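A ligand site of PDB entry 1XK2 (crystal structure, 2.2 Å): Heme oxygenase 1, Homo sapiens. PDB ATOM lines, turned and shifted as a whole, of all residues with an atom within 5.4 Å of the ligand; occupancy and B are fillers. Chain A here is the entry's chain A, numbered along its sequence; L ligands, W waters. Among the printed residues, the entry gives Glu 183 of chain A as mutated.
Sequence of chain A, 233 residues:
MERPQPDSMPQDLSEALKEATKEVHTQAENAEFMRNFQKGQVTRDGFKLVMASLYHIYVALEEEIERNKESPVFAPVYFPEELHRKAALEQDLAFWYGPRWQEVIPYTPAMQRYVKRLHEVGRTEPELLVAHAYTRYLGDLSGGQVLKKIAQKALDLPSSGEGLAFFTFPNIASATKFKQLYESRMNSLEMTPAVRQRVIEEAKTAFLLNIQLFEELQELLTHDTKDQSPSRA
The side-chain hydroxyl of Ser 142 lies within hydrogen-bond range of the backbone carbonyl oxygen of Leu 138 (3.1 Å). The guanidinium group of Arg 136 is in salt-bridge range of the side-chain carboxylate of Asp 140 (3.0 Å). The side-chain amide oxygen (OE1) of Gln 38 lies close to the backbone carbonyl oxygen (O) of Met 34. N of Lys 18 sits at hydrogen-bond distance from OH of Tyr 134 (3.5 Å). The side-chain amide oxygen of Asn 210 is in hydrogen-bond range of the guanidinium group of Arg 136 (3.0 Å). The side-chain amide oxygen (OE1) of Gln 38 lies close to the backbone carbonyl oxygen (O) of Glu 29, 3.0 Å away. The side-chain amide nitrogen (ND2) of Asn 210 is in hydrogen-bond range of the side-chain hydroxyl (OH) of Tyr 114 (3.2 Å). OH of Tyr 114 sits at hydrogen-bond distance from NH1 of Arg 136 (3.1 Å).
FE1 of the ligand is bound by NE2 of His 25 (2.1 Å). OG of Ser 142 lies within hydrogen-bond range of O2 of the ligand (3.0 Å). An oxygen (O1) of the ligand is in salt-bridge range of the side-chain amino group (NZ) of Lys 18. An oxygen (O4) of the ligand lies within hydrogen-bond range of the side-chain hydroxyl (OH) of Tyr 134 (2.6 Å).
Ala 28 touches the ligand. Glu 29 touches the ligand (CG to C18, 3.4 Å). Met 34 touches the ligand. Gln 38 touches the ligand (NE2 to C17, 3.1 Å). Thr 135 touches the ligand. Arg 136 touches the ligand (NH1 to C26, 3.4 Å). CA of Gly 139 touches C28 of the ligand (3.4 Å). Gly 143 touches the ligand (CA to C7, 3.6 Å). Leu 147 touches the ligand (CD2 to C14, 3.9 Å). Phe 207 touches the ligand. ND2 of Asn 210 touches C26 of the ligand, at 3.6 Å. Phe 214 touches the ligand (CE2 to C24, 3.6 Å). Within 4 Å of the ligand: Lys 18, His 25, Ala 28, Glu 29, Met 34, Gln 38, Tyr 134, Thr 135, Arg 136, Gly 139, Ser 142, Gly 143, Leu 147, Phe 207, Asn 210 and Phe 214. The nearest printed residue that does not touch the ligand is Val 146 (4.2 Å).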
ATOM      1  N   SER A  14      -7.184 -23.009 -32.595  1.00  0.00           N
ATOM      2  CA  SER A  14      -6.696 -22.041 -31.631  1.00  0.00           C
ATOM      3  C   SER A  14      -6.016 -20.873 -32.332  1.00  0.00           C
ATOM      4  O   SER A  14      -6.157 -19.724 -31.923  1.00  0.00           O
ATOM      5  CB  SER A  14      -5.726 -22.700 -30.645  1.00  0.00           C
ATOM      6  OG  SER A  14      -4.601 -23.244 -31.320  1.00  0.00           O
ATOM      7  N   LYS A  18      -7.624 -17.072 -32.246  1.00  0.00           N
ATOM      8  CA  LYS A  18      -6.766 -15.952 -31.887  1.00  0.00           C
ATOM      9  C   LYS A  18      -6.703 -14.861 -32.965  1.00  0.00           C
ATOM     10  O   LYS A  18      -6.704 -13.675 -32.657  1.00  0.00           O
ATOM     11  CB  LYS A  18      -5.359 -16.443 -31.568  1.00  0.00           C
ATOM     12  CG  LYS A  18      -4.345 -15.341 -31.320  1.00  0.00           C
ATOM     13  CD  LYS A  18      -2.971 -15.909 -31.015  1.00  0.00           C
ATOM     14  CE  LYS A  18      -1.930 -14.809 -30.914  1.00  0.00           C
ATOM     15  NZ  LYS A  18      -2.260 -13.834 -29.839  1.00  0.00           N
ATOM     16  N   HIS A  25     -10.892  -8.034 -29.652  1.00  0.00           N
ATOM     17  CA  HIS A  25     -10.096  -7.937 -28.431  1.00  0.00           C
ATOM     18  C   HIS A  25      -9.605  -6.507 -28.247  1.00  0.00           C
ATOM     19  O   HIS A  25      -9.705  -5.944 -27.147  1.00  0.00           O
ATOM     20  CB  HIS A  25      -8.910  -8.896 -28.484  1.00  0.00           C
ATOM     21  CG  HIS A  25      -8.156  -8.989 -27.189  1.00  0.00           C
ATOM     22  ND1 HIS A  25      -7.317  -7.984 -26.751  1.00  0.00           N
ATOM     23  CD2 HIS A  25      -8.175  -9.923 -26.215  1.00  0.00           C
ATOM     24  CE1 HIS A  25      -6.840  -8.301 -25.560  1.00  0.00           C
ATOM     25  NE2 HIS A  25      -7.346  -9.479 -25.211  1.00  0.00           N
ATOM     26  N   ALA A  28     -12.175  -4.570 -27.167  1.00  0.00           N
ATOM     27  CA  ALA A  28     -12.394  -4.778 -25.740  1.00  0.00           C
ATOM     28  C   ALA A  28     -11.479  -3.848 -24.950  1.00  0.00           C
ATOM     29  O   ALA A  28     -11.918  -3.179 -24.016  1.00  0.00           O
ATOM     30  CB  ALA A  28     -12.106  -6.240 -25.366  1.00  0.00           C
ATOM     31  N   GLU A  29     -10.212  -3.791 -25.339  1.00  0.00           N
ATOM     32  CA  GLU A  29      -9.248  -2.934 -24.666  1.00  0.00           C
ATOM     33  C   GLU A  29      -9.626  -1.470 -24.790  1.00  0.00           C
ATOM     34  O   GLU A  29      -9.367  -0.691 -23.883  1.00  0.00           O
ATOM     35  CB  GLU A  29      -7.851  -3.154 -25.249  1.00  0.00           C
ATOM     36  CG  GLU A  29      -7.365  -4.590 -25.139  1.00  0.00           C
ATOM     37  CD  GLU A  29      -6.142  -4.843 -25.977  1.00  0.00           C
ATOM     38  OE1 GLU A  29      -5.082  -4.252 -25.675  1.00  0.00           O
ATOM     39  OE2 GLU A  29      -6.232  -5.633 -26.934  1.00  0.00           O
ATOM     40  N   MET A  34     -12.804  -0.356 -19.593  1.00  0.00           N
ATOM     41  CA  MET A  34     -11.519  -1.047 -19.622  1.00  0.00           C
ATOM     42  C   MET A  34     -10.351  -0.103 -19.847  1.00  0.00           C
ATOM     43  O   MET A  34      -9.241  -0.408 -19.416  1.00  0.00           O
ATOM     44  CB  MET A  34     -11.544  -2.144 -20.687  1.00  0.00           C
ATOM     45  CG  MET A  34     -12.263  -3.406 -20.262  1.00  0.00           C
ATOM     46  SD  MET A  34     -11.382  -4.325 -18.960  1.00  0.00           S
ATOM     47  CE  MET A  34     -12.067  -3.598 -17.477  1.00  0.00           C
ATOM     48  N   GLN A  38      -7.217   0.300 -17.401  1.00  0.00           N
ATOM     49  CA  GLN A  38      -5.822   0.217 -17.846  1.00  0.00           C
ATOM     50  C   GLN A  38      -5.068   1.482 -17.438  1.00  0.00           C
ATOM     51  O   GLN A  38      -3.891   1.422 -17.088  1.00  0.00           O
ATOM     52  CB  GLN A  38      -5.761   0.049 -19.363  1.00  0.00           C
ATOM     53  CG  GLN A  38      -6.373  -1.258 -19.873  1.00  0.00           C
ATOM     54  CD  GLN A  38      -6.481  -1.334 -21.388  1.00  0.00           C
ATOM     55  OE1 GLN A  38      -7.021  -0.429 -22.021  1.00  0.00           O
ATOM     56  NE2 GLN A  38      -5.990  -2.412 -21.975  1.00  0.00           N
ATOM     57  N   TYR A 114     -25.378 -12.136 -21.080  1.00  0.00           N
ATOM     58  CA  TYR A 114     -24.212 -12.995 -21.193  1.00  0.00           C
ATOM     59  C   TYR A 114     -24.566 -14.391 -20.665  1.00  0.00           C
ATOM     60  O   TYR A 114     -24.369 -15.402 -21.351  1.00  0.00           O
ATOM     61  CB  TYR A 114     -23.076 -12.401 -20.371  1.00  0.00           C
ATOM     62  CG  TYR A 114     -21.683 -12.854 -20.759  1.00  0.00           C
ATOM     63  CD1 TYR A 114     -21.443 -14.131 -21.282  1.00  0.00           C
ATOM     64  CD2 TYR A 114     -20.592 -12.025 -20.515  1.00  0.00           C
ATOM     65  CE1 TYR A 114     -20.144 -14.564 -21.533  1.00  0.00           C
ATOM     66  CE2 TYR A 114     -19.295 -12.452 -20.754  1.00  0.00           C
ATOM     67  CZ  TYR A 114     -19.075 -13.719 -21.253  1.00  0.00           C
ATOM     68  OH  TYR A 114     -17.767 -14.126 -21.428  1.00  0.00           O
ATOM     69  N   TYR A 134     -12.843 -20.941 -24.069  1.00  0.00           N
ATOM     70  CA  TYR A 134     -11.632 -20.368 -24.637  1.00  0.00           C
ATOM     71  C   TYR A 134     -11.506 -18.890 -24.266  1.00  0.00           C
ATOM     72  O   TYR A 134     -10.507 -18.474 -23.685  1.00  0.00           O
ATOM     73  CB  TYR A 134     -11.660 -20.502 -26.152  1.00  0.00           C
ATOM     74  CG  TYR A 134     -10.654 -19.614 -26.858  1.00  0.00           C
ATOM     75  CD1 TYR A 134      -9.285 -19.857 -26.764  1.00  0.00           C
ATOM     76  CD2 TYR A 134     -11.084 -18.525 -27.615  1.00  0.00           C
ATOM     77  CE1 TYR A 134      -8.350 -19.028 -27.395  1.00  0.00           C
ATOM     78  CE2 TYR A 134     -10.157 -17.683 -28.262  1.00  0.00           C
ATOM     79  CZ  TYR A 134      -8.803 -17.944 -28.146  1.00  0.00           C
ATOM     80  OH  TYR A 134      -7.911 -17.129 -28.800  1.00  0.00           O
ATOM     81  N   THR A 135     -12.519 -18.117 -24.637  1.00  0.00           N
ATOM     82  CA  THR A 135     -12.572 -16.678 -24.399  1.00  0.00           C
ATOM     83  C   THR A 135     -12.386 -16.291 -22.933  1.00  0.00           C
ATOM     84  O   THR A 135     -11.631 -15.375 -22.614  1.00  0.00           O
ATOM     85  CB  THR A 135     -13.918 -16.102 -24.912  1.00  0.00           C
ATOM     86  OG1 THR A 135     -14.006 -16.287 -26.330  1.00  0.00           O
ATOM     87  CG2 THR A 135     -14.025 -14.611 -24.604  1.00  0.00           C
ATOM     88  N   ARG A 136     -13.075 -17.003 -22.038  1.00  0.00           N
ATOM     89  CA  ARG A 136     -12.973 -16.730 -20.606  1.00  0.00           C
ATOM     90  C   ARG A 136     -11.693 -17.266 -19.972  1.00  0.00           C
ATOM     91  O   ARG A 136     -10.788 -16.511 -19.630  1.00  0.00           O
ATOM     92  CB  ARG A 136     -14.177 -17.331 -19.872  1.00  0.00           C
ATOM     93  CG  ARG A 136     -15.409 -16.445 -19.805  1.00  0.00           C
ATOM     94  CD  ARG A 136     -15.495 -15.741 -18.464  1.00  0.00           C
ATOM     95  NE  ARG A 136     -14.444 -14.730 -18.269  1.00  0.00           N
ATOM     96  CZ  ARG A 136     -14.469 -13.516 -18.792  1.00  0.00           C
ATOM     97  NH1 ARG A 136     -15.495 -13.144 -19.555  1.00  0.00           N
ATOM     98  NH2 ARG A 136     -13.501 -12.652 -18.536  1.00  0.00           N
ATOM     99  N   LEU A 138      -8.887 -18.973 -21.068  1.00  0.00           N
ATOM    100  CA  LEU A 138      -7.604 -18.631 -21.662  1.00  0.00           C
ATOM    101  C   LEU A 138      -7.324 -17.140 -21.578  1.00  0.00           C
ATOM    102  O   LEU A 138      -6.187 -16.734 -21.340  1.00  0.00           O
ATOM    103  CB  LEU A 138      -7.551 -19.077 -23.121  1.00  0.00           C
ATOM    104  CG  LEU A 138      -6.524 -20.169 -23.385  1.00  0.00           C
ATOM    105  CD1 LEU A 138      -6.898 -21.429 -22.617  1.00  0.00           C
ATOM    106  CD2 LEU A 138      -6.447 -20.436 -24.882  1.00  0.00           C
ATOM    107  N   GLY A 139      -8.364 -16.331 -21.773  1.00  0.00           N
ATOM    108  CA  GLY A 139      -8.180 -14.901 -21.672  1.00  0.00           C
ATOM    109  C   GLY A 139      -7.772 -14.449 -20.278  1.00  0.00           C
ATOM    110  O   GLY A 139      -6.816 -13.691 -20.114  1.00  0.00           O
ATOM    111  N   ASP A 140      -8.503 -14.922 -19.269  1.00  0.00           N
ATOM    112  CA  ASP A 140      -8.203 -14.561 -17.884  1.00  0.00           C
ATOM    113  C   ASP A 140      -6.889 -15.150 -17.387  1.00  0.00           C
ATOM    114  O   ASP A 140      -6.318 -14.664 -16.408  1.00  0.00           O
ATOM    115  CB  ASP A 140      -9.334 -15.001 -16.950  1.00  0.00           C
ATOM    116  CG  ASP A 140     -10.632 -14.268 -17.230  1.00  0.00           C
ATOM    117  OD1 ASP A 140     -10.563 -13.113 -17.678  1.00  0.00           O
ATOM    118  OD2 ASP A 140     -11.709 -14.838 -16.980  1.00  0.00           O
ATOM    119  N   SER A 142      -3.969 -15.739 -19.480  1.00  0.00           N
ATOM    120  CA  SER A 142      -2.811 -15.088 -20.086  1.00  0.00           C
ATOM    121  C   SER A 142      -2.770 -13.599 -19.805  1.00  0.00           C
ATOM    122  O   SER A 142      -1.696 -12.990 -19.820  1.00  0.00           O
ATOM    123  CB  SER A 142      -2.804 -15.316 -21.605  1.00  0.00           C
ATOM    124  OG  SER A 142      -3.974 -14.783 -22.206  1.00  0.00           O
ATOM    125  N   GLY A 143      -3.923 -12.996 -19.537  1.00  0.00           N
ATOM    126  CA  GLY A 143      -3.957 -11.585 -19.251  1.00  0.00           C
ATOM    127  C   GLY A 143      -4.210 -11.305 -17.786  1.00  0.00           C
ATOM    128  O   GLY A 143      -4.212 -10.162 -17.345  1.00  0.00           O
ATOM    129  N   VAL A 146      -1.452  -9.052 -15.569  1.00  0.00           N
ATOM    130  CA  VAL A 146      -1.461  -7.622 -15.887  1.00  0.00           C
ATOM    131  C   VAL A 146      -2.708  -6.942 -15.345  1.00  0.00           C
ATOM    132  O   VAL A 146      -2.639  -5.819 -14.829  1.00  0.00           O
ATOM    133  CB  VAL A 146      -1.379  -7.368 -17.436  1.00  0.00           C
ATOM    134  CG1 VAL A 146      -0.339  -8.282 -18.066  1.00  0.00           C
ATOM    135  CG2 VAL A 146      -2.740  -7.564 -18.091  1.00  0.00           C
ATOM    136  N   LEU A 147      -3.851  -7.622 -15.447  1.00  0.00           N
ATOM    137  CA  LEU A 147      -5.118  -7.071 -14.971  1.00  0.00           C
ATOM    138  C   LEU A 147      -5.153  -6.985 -13.449  1.00  0.00           C
ATOM    139  O   LEU A 147      -5.712  -6.047 -12.890  1.00  0.00           O
ATOM    140  CB  LEU A 147      -6.284  -7.937 -15.470  1.00  0.00           C
ATOM    141  CG  LEU A 147      -6.365  -8.094 -17.005  1.00  0.00           C
ATOM    142  CD1 LEU A 147      -7.414  -9.125 -17.381  1.00  0.00           C
ATOM    143  CD2 LEU A 147      -6.673  -6.738 -17.631  1.00  0.00           C
ATOM    144  N   LYS A 179      -1.416 -23.366 -21.153  1.00  0.00           N
ATOM    145  CA  LYS A 179      -2.024 -22.687 -22.289  1.00  0.00           C
ATOM    146  C   LYS A 179      -1.835 -23.535 -23.551  1.00  0.00           C
ATOM    147  O   LYS A 179      -2.789 -23.828 -24.266  1.00  0.00           O
ATOM    148  CB  LYS A 179      -1.359 -21.322 -22.493  1.00  0.00           C
ATOM    149  CG  LYS A 179      -2.065 -20.429 -23.486  1.00  0.00           C
ATOM    150  CD  LYS A 179      -3.152 -19.598 -22.806  1.00  0.00           C
ATOM    151  CE  LYS A 179      -2.584 -18.428 -22.011  1.00  0.00           C
ATOM    152  NZ  LYS A 179      -1.750 -18.811 -20.823  1.00  0.00           N
ATOM    153  N   GLU A 183      -4.629 -25.496 -25.831  1.00  0.00           N
ATOM    154  CA  GLU A 183      -4.719 -25.235 -27.257  1.00  0.00           C
ATOM    155  C   GLU A 183      -4.639 -26.566 -27.991  1.00  0.00           C
ATOM    156  O   GLU A 183      -5.478 -26.877 -28.825  1.00  0.00           O
ATOM    157  CB  GLU A 183      -3.575 -24.322 -27.686  1.00  0.00           C
ATOM    158  CG  GLU A 183      -3.568 -23.035 -26.893  1.00  0.00           C
ATOM    159  CD  GLU A 183      -2.493 -22.089 -27.356  1.00  0.00           C
ATOM    160  OE1 GLU A 183      -1.390 -22.582 -27.694  1.00  0.00           O
ATOM    161  OE2 GLU A 183      -2.747 -20.868 -27.365  1.00  0.00           O
ATOM    162  N   PHE A 207     -16.824 -11.911 -27.111  1.00  0.00           N
ATOM    163  CA  PHE A 207     -16.207 -10.604 -26.903  1.00  0.00           C
ATOM    164  C   PHE A 207     -17.243  -9.479 -26.896  1.00  0.00           C
ATOM    165  O   PHE A 207     -17.139  -8.550 -26.094  1.00  0.00           O
ATOM    166  CB  PHE A 207     -15.145 -10.321 -27.985  1.00  0.00           C
ATOM    167  CG  PHE A 207     -13.837 -11.027 -27.756  1.00  0.00           C
ATOM    168  CD1 PHE A 207     -13.649 -12.331 -28.209  1.00  0.00           C
ATOM    169  CD2 PHE A 207     -12.805 -10.402 -27.059  1.00  0.00           C
ATOM    170  CE1 PHE A 207     -12.454 -13.000 -27.958  1.00  0.00           C
ATOM    171  CE2 PHE A 207     -11.606 -11.065 -26.804  1.00  0.00           C
ATOM    172  CZ  PHE A 207     -11.422 -12.376 -27.262  1.00  0.00           C
ATOM    173  N   ASN A 210     -19.010  -9.145 -23.601  1.00  0.00           N
ATOM    174  CA  ASN A 210     -18.163  -8.541 -22.579  1.00  0.00           C
ATOM    175  C   ASN A 210     -18.139  -7.030 -22.805  1.00  0.00           C
ATOM    176  O   ASN A 210     -18.240  -6.245 -21.857  1.00  0.00           O
ATOM    177  CB  ASN A 210     -16.750  -9.105 -22.677  1.00  0.00           C
ATOM    178  CG  ASN A 210     -16.634 -10.473 -22.048  1.00  0.00           C
ATOM    179  OD1 ASN A 210     -16.469 -10.595 -20.832  1.00  0.00           O
ATOM    180  ND2 ASN A 210     -16.710 -11.518 -22.876  1.00  0.00           N
ATOM    181  N   PHE A 214     -19.254  -4.100 -20.404  1.00  0.00           N
ATOM    182  CA  PHE A 214     -18.381  -3.009 -19.988  1.00  0.00           C
ATOM    183  C   PHE A 214     -19.097  -1.674 -20.191  1.00  0.00           C
ATOM    184  O   PHE A 214     -18.949  -0.759 -19.384  1.00  0.00           O
ATOM    185  CB  PHE A 214     -17.085  -2.985 -20.795  1.00  0.00           C
ATOM    186  CG  PHE A 214     -16.184  -4.160 -20.533  1.00  0.00           C
ATOM    187  CD1 PHE A 214     -16.184  -4.788 -19.295  1.00  0.00           C
ATOM    188  CD2 PHE A 214     -15.316  -4.613 -21.529  1.00  0.00           C
ATOM    189  CE1 PHE A 214     -15.329  -5.863 -19.050  1.00  0.00           C
ATOM    190  CE2 PHE A 214     -14.451  -5.671 -21.299  1.00  0.00           C
ATOM    191  CZ  PHE A 214     -14.450  -6.306 -20.050  1.00  0.00           C
HETATM  192  C1  LIG L   1      -5.043 -12.466 -24.417  1.00  0.00           C
HETATM  193  C2  LIG L   1      -4.796  -8.417 -21.728  1.00  0.00           C
HETATM  194  C3  LIG L   1      -9.573  -7.910 -22.082  1.00  0.00           C
HETATM  195  C4  LIG L   1      -9.848 -12.428 -23.935  1.00  0.00           C
HETATM  196  C5  LIG L   1      -4.540 -11.376 -23.687  1.00  0.00           C
HETATM  197  C6  LIG L   1      -3.130 -11.156 -23.348  1.00  0.00           C
HETATM  198  C7  LIG L   1      -3.107 -10.087 -22.469  1.00  0.00           C
HETATM  199  C8  LIG L   1      -4.474  -9.633 -22.317  1.00  0.00           C
HETATM  200  C9  LIG L   1      -1.899  -9.469 -21.753  1.00  0.00           C
HETATM  201  C10 LIG L   1      -1.850 -11.886 -23.797  1.00  0.00           C
HETATM  202  C11 LIG L   1      -1.615 -12.191 -25.269  1.00  0.00           C
HETATM  203  C12 LIG L   1      -2.108 -13.574 -25.676  1.00  0.00           C
HETATM  204  O1  LIG L   1      -2.068 -13.890 -26.891  1.00  0.00           O
HETATM  205  O2  LIG L   1      -2.529 -14.338 -24.788  1.00  0.00           O
HETATM  206  C13 LIG L   1      -6.050  -7.838 -21.798  1.00  0.00           C
HETATM  207  C14 LIG L   1      -6.327  -6.449 -21.487  1.00  0.00           C
HETATM  208  C15 LIG L   1      -7.652  -6.257 -21.709  1.00  0.00           C
HETATM  209  C16 LIG L   1      -8.219  -7.570 -22.058  1.00  0.00           C
HETATM  210  C17 LIG L   1      -5.338  -5.343 -21.118  1.00  0.00           C
HETATM  211  C18 LIG L   1      -8.146  -4.957 -21.864  1.00  0.00           C
HETATM  212  C19 LIG L   1      -9.487  -4.480 -21.624  1.00  0.00           C
HETATM  213  C20 LIG L   1     -10.060  -9.156 -22.485  1.00  0.00           C
HETATM  214  C21 LIG L   1     -11.457  -9.510 -22.531  1.00  0.00           C
HETATM  215  C22 LIG L   1     -11.533 -10.781 -22.991  1.00  0.00           C
HETATM  216  C23 LIG L   1     -10.172 -11.215 -23.297  1.00  0.00           C
HETATM  217  C24 LIG L   1     -12.649  -8.600 -22.224  1.00  0.00           C
HETATM  218  C25 LIG L   1     -12.699 -11.521 -23.122  1.00  0.00           C
HETATM  219  C26 LIG L   1     -13.285 -12.273 -22.041  1.00  0.00           C
HETATM  220  C27 LIG L   1      -8.572 -12.787 -24.331  1.00  0.00           C
HETATM  221  C28 LIG L   1      -8.221 -14.053 -24.971  1.00  0.00           C
HETATM  222  C29 LIG L   1      -6.873 -14.066 -25.106  1.00  0.00           C
HETATM  223  C30 LIG L   1      -6.386 -12.782 -24.595  1.00  0.00           C
HETATM  224  C31 LIG L   1      -9.137 -15.211 -25.343  1.00  0.00           C
HETATM  225  C32 LIG L   1      -6.004 -15.226 -25.582  1.00  0.00           C
HETATM  226  C33 LIG L   1      -6.063 -15.452 -27.087  1.00  0.00           C
HETATM  227  C34 LIG L   1      -5.028 -16.446 -27.582  1.00  0.00           C
HETATM  228  O3  LIG L   1      -3.820 -16.135 -27.485  1.00  0.00           O
HETATM  229  O4  LIG L   1      -5.417 -17.527 -28.070  1.00  0.00           O
HETATM  230  N1  LIG L   1      -5.357 -10.430 -23.057  1.00  0.00           N
HETATM  231  N2  LIG L   1      -7.196  -8.478 -22.279  1.00  0.00           N
HETATM  232  N3  LIG L   1      -9.263 -10.199 -22.981  1.00  0.00           N
HETATM  233  N4  LIG L   1      -7.424 -12.005 -24.103  1.00  0.00           N
HETATM  234 FE1  LIG L   1      -7.280 -10.208 -23.251  1.00  0.00          FE
HETATM  235  O   HOH W   1     -11.061 -13.479 -20.443  1.00  0.00           O
HETATM  236  O   HOH W   2      -8.610 -13.975 -28.795  1.00  0.00           O
